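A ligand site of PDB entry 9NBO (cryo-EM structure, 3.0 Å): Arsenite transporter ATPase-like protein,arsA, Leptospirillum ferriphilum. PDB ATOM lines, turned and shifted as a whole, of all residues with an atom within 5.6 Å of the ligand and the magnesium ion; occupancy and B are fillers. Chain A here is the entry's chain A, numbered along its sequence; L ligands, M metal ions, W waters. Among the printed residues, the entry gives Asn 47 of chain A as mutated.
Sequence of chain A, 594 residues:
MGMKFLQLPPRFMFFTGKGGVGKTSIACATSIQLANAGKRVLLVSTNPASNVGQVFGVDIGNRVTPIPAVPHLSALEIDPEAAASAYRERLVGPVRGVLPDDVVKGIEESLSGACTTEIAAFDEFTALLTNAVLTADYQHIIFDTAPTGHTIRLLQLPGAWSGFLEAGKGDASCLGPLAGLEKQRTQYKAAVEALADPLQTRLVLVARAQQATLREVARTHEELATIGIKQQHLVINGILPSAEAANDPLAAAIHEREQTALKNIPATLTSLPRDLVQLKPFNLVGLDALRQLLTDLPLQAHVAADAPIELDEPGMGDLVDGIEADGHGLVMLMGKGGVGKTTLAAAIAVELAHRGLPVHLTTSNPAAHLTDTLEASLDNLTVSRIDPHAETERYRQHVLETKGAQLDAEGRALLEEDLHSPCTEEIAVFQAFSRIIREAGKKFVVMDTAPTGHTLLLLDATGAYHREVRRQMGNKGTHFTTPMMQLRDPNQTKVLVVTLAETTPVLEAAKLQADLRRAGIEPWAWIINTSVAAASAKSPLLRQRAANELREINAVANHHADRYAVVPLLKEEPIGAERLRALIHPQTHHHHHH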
ATOM      1  N   LYS A  18      38.428 -20.794  27.625  1.00  0.00           N
ATOM      2  CA  LYS A  18      38.126 -22.158  28.036  1.00  0.00           C
ATOM      3  C   LYS A  18      37.265 -22.834  26.970  1.00  0.00           C
ATOM      4  O   LYS A  18      36.633 -22.178  26.149  1.00  0.00           O
ATOM      5  CB  LYS A  18      37.427 -22.147  29.392  1.00  0.00           C
ATOM      6  CG  LYS A  18      36.963 -23.495  29.888  1.00  0.00           C
ATOM      7  CD  LYS A  18      36.197 -23.362  31.183  1.00  0.00           C
ATOM      8  CE  LYS A  18      35.679 -24.704  31.635  1.00  0.00           C
ATOM      9  NZ  LYS A  18      34.645 -25.210  30.701  1.00  0.00           N
ATOM     10  N   GLY A  19      37.268 -24.157  26.979  1.00  0.00           N
ATOM     11  CA  GLY A  19      36.540 -24.891  25.960  1.00  0.00           C
ATOM     12  C   GLY A  19      35.041 -24.632  26.043  1.00  0.00           C
ATOM     13  O   GLY A  19      34.478 -24.479  27.131  1.00  0.00           O
ATOM     14  N   GLY A  20      34.401 -24.565  24.881  1.00  0.00           N
ATOM     15  CA  GLY A  20      32.960 -24.460  24.790  1.00  0.00           C
ATOM     16  C   GLY A  20      32.383 -23.101  25.065  1.00  0.00           C
ATOM     17  O   GLY A  20      31.163 -22.964  25.107  1.00  0.00           O
ATOM     18  N   VAL A  21      33.231 -22.079  25.246  1.00  0.00           N
ATOM     19  CA  VAL A  21      32.721 -20.754  25.615  1.00  0.00           C
ATOM     20  C   VAL A  21      32.147 -19.997  24.420  1.00  0.00           C
ATOM     21  O   VAL A  21      31.354 -19.075  24.619  1.00  0.00           O
ATOM     22  CB  VAL A  21      33.836 -19.916  26.273  1.00  0.00           C
ATOM     23  CG1 VAL A  21      34.242 -20.532  27.591  1.00  0.00           C
ATOM     24  CG2 VAL A  21      35.024 -19.760  25.336  1.00  0.00           C
ATOM     25  N   GLY A  22      32.524 -20.352  23.202  1.00  0.00           N
ATOM     26  CA  GLY A  22      32.022 -19.672  22.027  1.00  0.00           C
ATOM     27  C   GLY A  22      33.103 -19.002  21.212  1.00  0.00           C
ATOM     28  O   GLY A  22      32.850 -18.017  20.520  1.00  0.00           O
ATOM     29  N   LYS A  23      34.323 -19.534  21.284  1.00  0.00           N
ATOM     30  CA  LYS A  23      35.423 -18.963  20.497  1.00  0.00           C
ATOM     31  C   LYS A  23      35.148 -19.084  19.010  1.00  0.00           C
ATOM     32  O   LYS A  23      35.324 -18.123  18.251  1.00  0.00           O
ATOM     33  CB  LYS A  23      36.739 -19.644  20.842  1.00  0.00           C
ATOM     34  CG  LYS A  23      36.982 -19.868  22.315  1.00  0.00           C
ATOM     35  CD  LYS A  23      38.321 -20.520  22.549  1.00  0.00           C
ATOM     36  CE  LYS A  23      38.247 -22.017  22.324  1.00  0.00           C
ATOM     37  NZ  LYS A  23      37.554 -22.678  23.456  1.00  0.00           N
ATOM     38  N   THR A  24      34.716 -20.271  18.558  1.00  0.00           N
ATOM     39  CA  THR A  24      34.471 -20.471  17.131  1.00  0.00           C
ATOM     40  C   THR A  24      33.279 -19.648  16.657  1.00  0.00           C
ATOM     41  O   THR A  24      33.335 -19.035  15.588  1.00  0.00           O
ATOM     42  CB  THR A  24      34.237 -21.949  16.855  1.00  0.00           C
ATOM     43  OG1 THR A  24      35.378 -22.704  17.271  1.00  0.00           O
ATOM     44  CG2 THR A  24      34.004 -22.181  15.371  1.00  0.00           C
ATOM     45  N   SER A  25      32.204 -19.618  17.442  1.00  0.00           N
ATOM     46  CA  SER A  25      31.025 -18.859  17.037  1.00  0.00           C
ATOM     47  C   SER A  25      31.351 -17.375  16.911  1.00  0.00           C
ATOM     48  O   SER A  25      31.013 -16.731  15.917  1.00  0.00           O
ATOM     49  CB  SER A  25      29.892 -19.077  18.040  1.00  0.00           C
ATOM     50  OG  SER A  25      29.394 -20.397  17.947  1.00  0.00           O
ATOM     51  N   ILE A  26      32.025 -16.822  17.923  1.00  0.00           N
ATOM     52  CA  ILE A  26      32.339 -15.395  17.921  1.00  0.00           C
ATOM     53  C   ILE A  26      33.368 -15.075  16.846  1.00  0.00           C
ATOM     54  O   ILE A  26      33.305 -14.026  16.206  1.00  0.00           O
ATOM     55  CB  ILE A  26      32.801 -14.955  19.320  1.00  0.00           C
ATOM     56  CG1 ILE A  26      31.663 -15.128  20.323  1.00  0.00           C
ATOM     57  CG2 ILE A  26      33.270 -13.516  19.304  1.00  0.00           C
ATOM     58  CD1 ILE A  26      32.042 -14.850  21.751  1.00  0.00           C
ATOM     59  N   ASN A  47      41.961 -25.525  15.942  1.00  0.00           N
ATOM     60  CA  ASN A  47      41.439 -26.634  16.720  1.00  0.00           C
ATOM     61  C   ASN A  47      41.396 -27.876  15.830  1.00  0.00           C
ATOM     62  O   ASN A  47      40.598 -27.905  14.880  1.00  0.00           O
ATOM     63  CB  ASN A  47      40.061 -26.314  17.258  1.00  0.00           C
ATOM     64  CG  ASN A  47      39.648 -27.219  18.399  1.00  0.00           C
ATOM     65  OD1 ASN A  47      40.409 -28.090  18.814  1.00  0.00           O
ATOM     66  ND2 ASN A  47      38.447 -27.020  18.909  1.00  0.00           N
ATOM     67  N   SER A  50      37.717 -29.645  15.606  1.00  0.00           N
ATOM     68  CA  SER A  50      36.555 -28.916  15.128  1.00  0.00           C
ATOM     69  C   SER A  50      36.607 -28.757  13.612  1.00  0.00           C
ATOM     70  O   SER A  50      37.661 -28.835  12.985  1.00  0.00           O
ATOM     71  CB  SER A  50      36.449 -27.540  15.783  1.00  0.00           C
ATOM     72  OG  SER A  50      36.150 -27.666  17.161  1.00  0.00           O
ATOM     73  N   ASP A 144      41.028 -18.870  15.478  1.00  0.00           N
ATOM     74  CA  ASP A 144      40.092 -19.523  16.388  1.00  0.00           C
ATOM     75  C   ASP A 144      40.794 -20.735  16.980  1.00  0.00           C
ATOM     76  O   ASP A 144      40.987 -21.746  16.307  1.00  0.00           O
ATOM     77  CB  ASP A 144      38.816 -19.924  15.662  1.00  0.00           C
ATOM     78  CG  ASP A 144      37.867 -20.676  16.563  1.00  0.00           C
ATOM     79  OD1 ASP A 144      37.409 -20.084  17.559  1.00  0.00           O
ATOM     80  OD2 ASP A 144      37.575 -21.850  16.260  1.00  0.00           O
ATOM     81  N   THR A 145      41.160 -20.639  18.254  1.00  0.00           N
ATOM     82  CA  THR A 145      42.066 -21.592  18.873  1.00  0.00           C
ATOM     83  C   THR A 145      41.301 -22.728  19.547  1.00  0.00           C
ATOM     84  O   THR A 145      40.077 -22.687  19.685  1.00  0.00           O
ATOM     85  CB  THR A 145      42.975 -20.880  19.875  1.00  0.00           C
ATOM     86  OG1 THR A 145      42.166 -20.248  20.876  1.00  0.00           O
ATOM     87  CG2 THR A 145      43.818 -19.824  19.173  1.00  0.00           C
ATOM     88  N   ALA A 146      42.048 -23.746  19.970  1.00  0.00           N
ATOM     89  CA  ALA A 146      41.513 -24.858  20.742  1.00  0.00           C
ATOM     90  C   ALA A 146      41.261 -24.391  22.163  1.00  0.00           C
ATOM     91  O   ALA A 146      41.636 -23.265  22.515  1.00  0.00           O
ATOM     92  CB  ALA A 146      42.484 -26.035  20.704  1.00  0.00           C
ATOM     93  N   PRO A 147      40.638 -25.205  23.021  1.00  0.00           N
ATOM     94  CA  PRO A 147      40.439 -24.771  24.419  1.00  0.00           C
ATOM     95  C   PRO A 147      41.728 -24.275  25.047  1.00  0.00           C
ATOM     96  O   PRO A 147      42.822 -24.605  24.581  1.00  0.00           O
ATOM     97  CB  PRO A 147      39.912 -26.040  25.099  1.00  0.00           C
ATOM     98  CG  PRO A 147      39.238 -26.783  24.018  1.00  0.00           C
ATOM     99  CD  PRO A 147      40.034 -26.522  22.782  1.00  0.00           C
ATOM    100  N   ARG A 208      32.290 -17.417  29.973  1.00  0.00           N
ATOM    101  CA  ARG A 208      30.866 -17.452  30.241  1.00  0.00           C
ATOM    102  C   ARG A 208      30.618 -16.988  31.675  1.00  0.00           C
ATOM    103  O   ARG A 208      31.527 -16.983  32.514  1.00  0.00           O
ATOM    104  CB  ARG A 208      30.292 -18.856  30.030  1.00  0.00           C
ATOM    105  CG  ARG A 208      30.235 -19.290  28.578  1.00  0.00           C
ATOM    106  CD  ARG A 208      29.032 -20.192  28.320  1.00  0.00           C
ATOM    107  NE  ARG A 208      29.192 -20.978  27.097  1.00  0.00           N
ATOM    108  CZ  ARG A 208      28.365 -20.961  26.068  1.00  0.00           C
ATOM    109  NH1 ARG A 208      27.279 -20.215  26.052  1.00  0.00           N
ATOM    110  NH2 ARG A 208      28.640 -21.726  25.012  1.00  0.00           N
ATOM    111  N   ASN A 237      29.965 -14.654  27.067  1.00  0.00           N
ATOM    112  CA  ASN A 237      29.015 -15.209  26.120  1.00  0.00           C
ATOM    113  C   ASN A 237      27.982 -16.066  26.846  1.00  0.00           C
ATOM    114  O   ASN A 237      28.202 -16.513  27.972  1.00  0.00           O
ATOM    115  CB  ASN A 237      29.746 -16.044  25.074  1.00  0.00           C
ATOM    116  CG  ASN A 237      28.867 -16.412  23.904  1.00  0.00           C
ATOM    117  OD1 ASN A 237      27.687 -16.087  23.868  1.00  0.00           O
ATOM    118  ND2 ASN A 237      29.447 -17.080  22.922  1.00  0.00           N
ATOM    119  N   GLY A 238      26.844 -16.266  26.194  1.00  0.00           N
ATOM    120  CA  GLY A 238      25.808 -17.099  26.760  1.00  0.00           C
ATOM    121  C   GLY A 238      25.091 -16.489  27.936  1.00  0.00           C
ATOM    122  O   GLY A 238      24.529 -17.217  28.756  1.00  0.00           O
ATOM    123  N   VAL A 277      27.665 -10.935  25.276  1.00  0.00           N
ATOM    124  CA  VAL A 277      26.921 -11.611  24.217  1.00  0.00           C
ATOM    125  C   VAL A 277      25.848 -12.452  24.875  1.00  0.00           C
ATOM    126  O   VAL A 277      26.140 -13.249  25.769  1.00  0.00           O
ATOM    127  CB  VAL A 277      27.834 -12.459  23.332  1.00  0.00           C
ATOM    128  CG1 VAL A 277      27.032 -13.176  22.269  1.00  0.00           C
ATOM    129  CG2 VAL A 277      28.913 -11.608  22.690  1.00  0.00           C
ATOM    130  N   GLN A 278      24.606 -12.279  24.440  1.00  0.00           N
ATOM    131  CA  GLN A 278      23.479 -12.947  25.063  1.00  0.00           C
ATOM    132  C   GLN A 278      23.341 -14.374  24.525  1.00  0.00           C
ATOM    133  O   GLN A 278      24.029 -14.803  23.607  1.00  0.00           O
ATOM    134  CB  GLN A 278      22.190 -12.175  24.812  1.00  0.00           C
ATOM    135  CG  GLN A 278      22.084 -10.883  25.603  1.00  0.00           C
ATOM    136  CD  GLN A 278      20.747 -10.210  25.404  1.00  0.00           C
ATOM    137  OE1 GLN A 278      20.027 -10.497  24.458  1.00  0.00           O
ATOM    138  NE2 GLN A 278      20.412  -9.295  26.308  1.00  0.00           N
ATOM    139  N   LEU A 279      22.424 -15.123  25.145  1.00  0.00           N
ATOM    140  CA  LEU A 279      22.083 -16.461  24.702  1.00  0.00           C
ATOM    141  C   LEU A 279      21.018 -16.382  23.625  1.00  0.00           C
ATOM    142  O   LEU A 279      20.047 -15.630  23.747  1.00  0.00           O
ATOM    143  CB  LEU A 279      21.581 -17.306  25.875  1.00  0.00           C
ATOM    144  CG  LEU A 279      21.517 -18.813  25.652  1.00  0.00           C
ATOM    145  CD1 LEU A 279      22.900 -19.428  25.665  1.00  0.00           C
ATOM    146  CD2 LEU A 279      20.645 -19.451  26.701  1.00  0.00           C
ATOM    147  N   LYS A 280      21.205 -17.158  22.557  1.00  0.00           N
ATOM    148  CA  LYS A 280      20.307 -17.125  21.423  1.00  0.00           C
ATOM    149  C   LYS A 280      19.454 -18.387  21.387  1.00  0.00           C
ATOM    150  O   LYS A 280      19.896 -19.449  21.824  1.00  0.00           O
ATOM    151  CB  LYS A 280      21.082 -17.009  20.098  1.00  0.00           C
ATOM    152  CG  LYS A 280      22.213 -15.990  20.106  1.00  0.00           C
ATOM    153  CD  LYS A 280      21.688 -14.590  19.862  1.00  0.00           C
ATOM    154  CE  LYS A 280      22.663 -13.533  20.354  1.00  0.00           C
ATOM    155  NZ  LYS A 280      21.984 -12.260  20.669  1.00  0.00           N
ATOM    156  N   PHE A 282      18.790 -20.240  18.977  1.00  0.00           N
ATOM    157  CA  PHE A 282      19.146 -21.064  17.829  1.00  0.00           C
ATOM    158  C   PHE A 282      20.623 -21.419  17.922  1.00  0.00           C
ATOM    159  O   PHE A 282      21.426 -20.671  18.477  1.00  0.00           O
ATOM    160  CB  PHE A 282      18.870 -20.334  16.517  1.00  0.00           C
ATOM    161  CG  PHE A 282      19.346 -18.909  16.494  1.00  0.00           C
ATOM    162  CD1 PHE A 282      20.698 -18.625  16.385  1.00  0.00           C
ATOM    163  CD2 PHE A 282      18.447 -17.865  16.574  1.00  0.00           C
ATOM    164  CE1 PHE A 282      21.133 -17.322  16.377  1.00  0.00           C
ATOM    165  CE2 PHE A 282      18.888 -16.559  16.550  1.00  0.00           C
ATOM    166  CZ  PHE A 282      20.231 -16.292  16.454  1.00  0.00           C
ATOM    167  N   ASN A 283      20.967 -22.571  17.351  1.00  0.00           N
ATOM    168  CA  ASN A 283      22.366 -22.974  17.268  1.00  0.00           C
ATOM    169  C   ASN A 283      23.094 -22.080  16.277  1.00  0.00           C
ATOM    170  O   ASN A 283      22.574 -21.754  15.210  1.00  0.00           O
ATOM    171  CB  ASN A 283      22.471 -24.429  16.856  1.00  0.00           C
ATOM    172  CG  ASN A 283      22.311 -25.377  18.016  1.00  0.00           C
ATOM    173  OD1 ASN A 283      22.673 -25.048  19.152  1.00  0.00           O
ATOM    174  ND2 ASN A 283      21.766 -26.558  17.747  1.00  0.00           N
ATOM    175  N   LEU A 284      24.323 -21.686  16.634  1.00  0.00           N
ATOM    176  CA  LEU A 284      25.105 -20.761  15.811  1.00  0.00           C
ATOM    177  C   LEU A 284      25.765 -21.525  14.675  1.00  0.00           C
ATOM    178  O   LEU A 284      26.974 -21.738  14.622  1.00  0.00           O
ATOM    179  CB  LEU A 284      26.133 -20.038  16.679  1.00  0.00           C
ATOM    180  CG  LEU A 284      25.615 -18.848  17.497  1.00  0.00           C
ATOM    181  CD1 LEU A 284      25.172 -17.714  16.602  1.00  0.00           C
ATOM    182  CD2 LEU A 284      24.486 -19.267  18.411  1.00  0.00           C
ATOM    183  N   LEU A 293      24.666 -12.880  15.961  1.00  0.00           N
ATOM    184  CA  LEU A 293      25.214 -13.326  17.236  1.00  0.00           C
ATOM    185  C   LEU A 293      25.680 -12.168  18.096  1.00  0.00           C
ATOM    186  O   LEU A 293      25.505 -12.200  19.325  1.00  0.00           O
ATOM    187  CB  LEU A 293      26.377 -14.298  16.993  1.00  0.00           C
ATOM    188  CG  LEU A 293      27.251 -14.638  18.198  1.00  0.00           C
ATOM    189  CD1 LEU A 293      26.428 -15.230  19.324  1.00  0.00           C
ATOM    190  CD2 LEU A 293      28.349 -15.598  17.801  1.00  0.00           C
ATOM    191  N   LYS A 336      33.675 -32.945  22.999  1.00  0.00           N
ATOM    192  CA  LYS A 336      33.954 -31.568  22.613  1.00  0.00           C
ATOM    193  C   LYS A 336      34.257 -30.731  23.857  1.00  0.00           C
ATOM    194  O   LYS A 336      33.919 -31.099  24.979  1.00  0.00           O
ATOM    195  CB  LYS A 336      32.776 -30.982  21.848  1.00  0.00           C
ATOM    196  CG  LYS A 336      33.018 -29.588  21.294  1.00  0.00           C
ATOM    197  CD  LYS A 336      31.861 -29.132  20.440  1.00  0.00           C
ATOM    198  CE  LYS A 336      32.013 -27.680  20.055  1.00  0.00           C
ATOM    199  NZ  LYS A 336      32.104 -26.806  21.244  1.00  0.00           N
ATOM    200  N   GLY A 337      34.915 -29.594  23.636  1.00  0.00           N
ATOM    201  CA  GLY A 337      35.236 -28.714  24.751  1.00  0.00           C
ATOM    202  C   GLY A 337      33.978 -28.136  25.385  1.00  0.00           C
ATOM    203  O   GLY A 337      33.016 -27.791  24.697  1.00  0.00           O
ATOM    204  N   GLY A 338      34.001 -28.033  26.705  1.00  0.00           N
ATOM    205  CA  GLY A 338      32.925 -27.417  27.445  1.00  0.00           C
ATOM    206  C   GLY A 338      31.687 -28.260  27.615  1.00  0.00           C
ATOM    207  O   GLY A 338      30.685 -27.765  28.157  1.00  0.00           O
ATOM    208  N   LEU A 500      26.735 -32.322  23.940  1.00  0.00           N
ATOM    209  CA  LEU A 500      25.627 -31.428  24.222  1.00  0.00           C
ATOM    210  C   LEU A 500      24.541 -31.698  23.202  1.00  0.00           C
ATOM    211  O   LEU A 500      24.823 -32.149  22.089  1.00  0.00           O
ATOM    212  CB  LEU A 500      26.062 -29.963  24.153  1.00  0.00           C
ATOM    213  CG  LEU A 500      27.108 -29.487  25.174  1.00  0.00           C
ATOM    214  CD1 LEU A 500      27.589 -28.097  24.829  1.00  0.00           C
ATOM    215  CD2 LEU A 500      26.531 -29.507  26.565  1.00  0.00           C
ATOM    216  N   GLU A 502      23.207 -30.361  20.886  1.00  0.00           N
ATOM    217  CA  GLU A 502      23.356 -29.289  19.924  1.00  0.00           C
ATOM    218  C   GLU A 502      24.050 -29.835  18.682  1.00  0.00           C
ATOM    219  O   GLU A 502      24.685 -30.892  18.706  1.00  0.00           O
ATOM    220  CB  GLU A 502      24.128 -28.103  20.498  1.00  0.00           C
ATOM    221  CG  GLU A 502      23.435 -27.429  21.663  1.00  0.00           C
ATOM    222  CD  GLU A 502      24.339 -26.479  22.416  1.00  0.00           C
ATOM    223  OE1 GLU A 502      25.498 -26.847  22.680  1.00  0.00           O
ATOM    224  OE2 GLU A 502      23.890 -25.356  22.749  1.00  0.00           O
ATOM    225  N   THR A 503      23.924 -29.086  17.586  1.00  0.00           N
ATOM    226  CA  THR A 503      24.400 -29.573  16.290  1.00  0.00           C
ATOM    227  C   THR A 503      25.898 -29.849  16.316  1.00  0.00           C
ATOM    228  O   THR A 503      26.333 -30.990  16.157  1.00  0.00           O
ATOM    229  CB  THR A 503      24.056 -28.544  15.203  1.00  0.00           C
ATOM    230  OG1 THR A 503      22.638 -28.405  15.108  1.00  0.00           O
ATOM    231  CG2 THR A 503      24.608 -28.982  13.862  1.00  0.00           C
ATOM    232  N   THR A 504      26.697 -28.805  16.502  1.00  0.00           N
ATOM    233  CA  THR A 504      28.140 -28.913  16.386  1.00  0.00           C
ATOM    234  C   THR A 504      28.714 -29.865  17.442  1.00  0.00           C
ATOM    235  O   THR A 504      29.588 -30.670  17.118  1.00  0.00           O
ATOM    236  CB  THR A 504      28.797 -27.538  16.499  1.00  0.00           C
ATOM    237  OG1 THR A 504      28.553 -26.802  15.294  1.00  0.00           O
ATOM    238  CG2 THR A 504      30.294 -27.676  16.686  1.00  0.00           C
ATOM    239  N   PRO A 505      28.289 -29.787  18.707  1.00  0.00           N
ATOM    240  CA  PRO A 505      28.772 -30.769  19.680  1.00  0.00           C
ATOM    241  C   PRO A 505      28.478 -32.211  19.293  1.00  0.00           C
ATOM    242  O   PRO A 505      29.331 -33.083  19.457  1.00  0.00           O
ATOM    243  CB  PRO A 505      28.064 -30.372  20.967  1.00  0.00           C
ATOM    244  CG  PRO A 505      27.812 -28.925  20.816  1.00  0.00           C
ATOM    245  CD  PRO A 505      27.532 -28.714  19.365  1.00  0.00           C
ATOM    246  N   GLU A 508      30.779 -33.187  16.374  1.00  0.00           N
ATOM    247  CA  GLU A 508      32.136 -33.384  16.855  1.00  0.00           C
ATOM    248  C   GLU A 508      32.265 -34.684  17.633  1.00  0.00           C
ATOM    249  O   GLU A 508      33.266 -35.393  17.524  1.00  0.00           O
ATOM    250  CB  GLU A 508      32.566 -32.200  17.724  1.00  0.00           C
ATOM    251  CG  GLU A 508      34.024 -32.218  18.123  1.00  0.00           C
ATOM    252  CD  GLU A 508      34.596 -30.837  18.336  1.00  0.00           C
ATOM    253  OE1 GLU A 508      34.200 -29.906  17.606  1.00  0.00           O
ATOM    254  OE2 GLU A 508      35.455 -30.674  19.233  1.00  0.00           O
ATOM    255  N   ARG A 545      15.083 -23.507  22.840  1.00  0.00           N
ATOM    256  CA  ARG A 545      16.317 -24.277  22.939  1.00  0.00           C
ATOM    257  C   ARG A 545      16.026 -25.757  23.147  1.00  0.00           C
ATOM    258  O   ARG A 545      16.660 -26.609  22.524  1.00  0.00           O
ATOM    259  CB  ARG A 545      17.192 -23.728  24.063  1.00  0.00           C
ATOM    260  CG  ARG A 545      17.617 -22.281  23.863  1.00  0.00           C
ATOM    261  CD  ARG A 545      18.954 -21.968  24.510  1.00  0.00           C
ATOM    262  NE  ARG A 545      20.067 -22.117  23.575  1.00  0.00           N
ATOM    263  CZ  ARG A 545      20.963 -23.097  23.604  1.00  0.00           C
ATOM    264  NH1 ARG A 545      20.891 -24.073  24.506  1.00  0.00           N
ATOM    265  NH2 ARG A 545      21.936 -23.113  22.714  1.00  0.00           N
HETATM  266  P1  LIG L   1      35.804 -25.703  21.431  1.00  0.00           P
HETATM  267  O1  LIG L   1      35.325 -27.103  21.538  1.00  0.00           O
HETATM  268  O2  LIG L   1      36.608 -25.233  22.628  1.00  0.00           O
HETATM  269  O3  LIG L   1      36.595 -25.413  20.168  1.00  0.00           O
HETATM  270  P2  LIG L   1      34.269 -23.194  21.013  1.00  0.00           P
HETATM  271  O4  LIG L   1      34.851 -22.279  22.000  1.00  0.00           O
HETATM  272  O5  LIG L   1      34.681 -22.998  19.564  1.00  0.00           O
HETATM  273  O6  LIG L   1      34.574 -24.705  21.366  1.00  0.00           O
HETATM  274  P3  LIG L   1      31.490 -23.193  20.017  1.00  0.00           P
HETATM  275  O7  LIG L   1      31.592 -24.325  19.083  1.00  0.00           O
HETATM  276  O8  LIG L   1      31.444 -21.824  19.350  1.00  0.00           O
HETATM  277  O9  LIG L   1      32.681 -23.169  21.059  1.00  0.00           O
HETATM  278  O10 LIG L   1      30.237 -23.311  20.966  1.00  0.00           O
HETATM  279  C1  LIG L   1      29.655 -24.595  21.285  1.00  0.00           C
HETATM  280  C2  LIG L   1      28.172 -24.427  21.208  1.00  0.00           C
HETATM  281  O11 LIG L   1      27.891 -23.153  21.805  1.00  0.00           O
HETATM  282  C3  LIG L   1      27.737 -24.275  19.750  1.00  0.00           C
HETATM  283  O12 LIG L   1      26.772 -25.294  19.525  1.00  0.00           O
HETATM  284  C4  LIG L   1      26.958 -22.959  19.710  1.00  0.00           C
HETATM  285  O13 LIG L   1      25.662 -23.301  19.248  1.00  0.00           O
HETATM  286  C5  LIG L   1      26.759 -22.631  21.183  1.00  0.00           C
HETATM  287  N1  LIG L   1      26.799 -21.197  21.423  1.00  0.00           N
HETATM  288  C6  LIG L   1      27.909 -20.408  21.514  1.00  0.00           C
HETATM  289  N2  LIG L   1      27.664 -19.149  21.741  1.00  0.00           N
HETATM  290  C7  LIG L   1      26.274 -19.090  21.806  1.00  0.00           C
HETATM  291  C8  LIG L   1      25.372 -18.032  22.012  1.00  0.00           C
HETATM  292  N3  LIG L   1      25.751 -16.770  22.219  1.00  0.00           N
HETATM  293  N4  LIG L   1      24.061 -18.319  22.011  1.00  0.00           N
HETATM  294  C9  LIG L   1      23.673 -19.589  21.812  1.00  0.00           C
HETATM  295  N5  LIG L   1      24.433 -20.663  21.593  1.00  0.00           N
HETATM  296  C10 LIG L   1      25.731 -20.347  21.606  1.00  0.00           C
HETATM  297 MG    MG M   1      36.304 -23.947  18.349  1.00  0.00          MG
HETATM  298  O   HOH W   1      37.165 -29.329  20.470  1.00  0.00           O
HETATM  299  O   HOH W   2      30.951 -26.883  23.438  1.00  0.00           O
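ND2 of Asn 237 sits at hydrogen-bond distance from O of Val 21 (3.2 Å). The side-chain amide nitrogen of Asn 47 lies within hydrogen-bond range of the side-chain hydroxyl of Ser 50, at 3.0 Å. NZ of Lys 23 lies within hydrogen-bond range of O of Lys 18, 2.9 Å away. The backbone carbonyl oxygen of Lys 280 is in hydrogen-bond range of the guanidinium group of Arg 545 (3.2 Å). The side-chain amide nitrogen (ND2) of Asn 283 lies close to the backbone NH (N) of Thr 503, 3.3 Å away. The guanidinium group (NH2) of Arg 545 lies within salt-bridge range of the side-chain carboxylate (OE2) of Glu 502 (3.0 Å). OE1 of Glu 508 lies within hydrogen-bond range of OG of Ser 50 (3.0 Å). O of Val 277 is in hydrogen-bond range of N of Gly 238, at 3.1 Å.
Residues that only touch the magnesium ion: Asp 144 (3.2 Å), Asn 47 (3.8 Å) and Ser 50 (3.9 Å).
N of Thr 24 sits close to O5 of the ligand, at 2.9 Å. The side-chain amide oxygen (OD1) of Asn 237 lies within hydrogen-bond range of a nitrogen (N3) of the ligand (2.6 Å). ND2 of Asn 47 sits close to O3 of the ligand, at 2.8 Å. N of Lys 23 sits at hydrogen-bond distance from O4 of the ligand. The side-chain amino group (NZ) of Lys 23 is in salt-bridge range of an oxygen (O2) of the ligand. The backbone NH (N) of Ser 25 sits at hydrogen-bond distance from an oxygen (O8) of the ligand (3.0 Å). The side-chain hydroxyl of Ser 25 is in hydrogen-bond range of an oxygen (O8) of the ligand. N3 of the ligand sits at hydrogen-bond distance from O of Gln 278 (3.0 Å). A nitrogen (N4) of the ligand lies within hydrogen-bond range of the backbone NH (N) of Lys 280 (3.1 Å). The backbone NH of Gly 20 lies within hydrogen-bond range of an oxygen (O2) of the ligand. NZ of Lys 336 lies within salt-bridge range of O1 of the ligand (3.2 Å). N of Gly 22 sits at hydrogen-bond distance from O4 of the ligand (3.3 Å). An oxygen (O1) of the ligand sits at hydrogen-bond distance from the backbone NH (N) of Gly 337. O13 of the ligand sits at hydrogen-bond distance from N of Leu 284, 3.4 Å away. The side-chain amide oxygen (OD1) of Asn 283 lies within hydrogen-bond range of an oxygen (O13) of the ligand.
CA of Gly 19 touches O2 of the ligand, at 3.4 Å. Val 21 touches the ligand. Ser 50 touches the ligand (OG to O3, 3.8 Å). CG of Pro 147 touches O2 of the ligand (3.4 Å). Arg 208 touches the ligand. Val 277 touches the ligand. Leu 279 touches the ligand (CA to N4, 3.8 Å). Leu 293 touches the ligand. Glu 502 touches the ligand. Pro 505 touches the ligand. Arg 545 touches the ligand (NH2 to N5, 3.7 Å). Hydrophobic or aromatic side chains that line the ligand: Pro 147, Val 277, Leu 279, Leu 284, Leu 293 and Pro 505. Of the 36 residues printed, 24 come within 4 Å of the ligand. The nearest printed residue that does not touch the ligand is Gly 238 (4.2 Å).
Water W1 lies within hydrogen-bond range of the side-chain carboxylate of Glu 508 (2.5 Å), the side-chain amide nitrogen of Asn 47 (3.1 Å) and an oxygen (O1) of the ligand (3.1 Å). Water W2 lies within hydrogen-bond range of NZ of Lys 336 (2.5 Å) and O of Gly 337 (2.6 Å).
The magnesium ion is bound by OG1 of Thr 24 (1.9 Å), O5 of the ligand (2.2 Å) and O3 of the ligand (2.4 Å). The magnesium ion has three donor atoms within binding distance.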
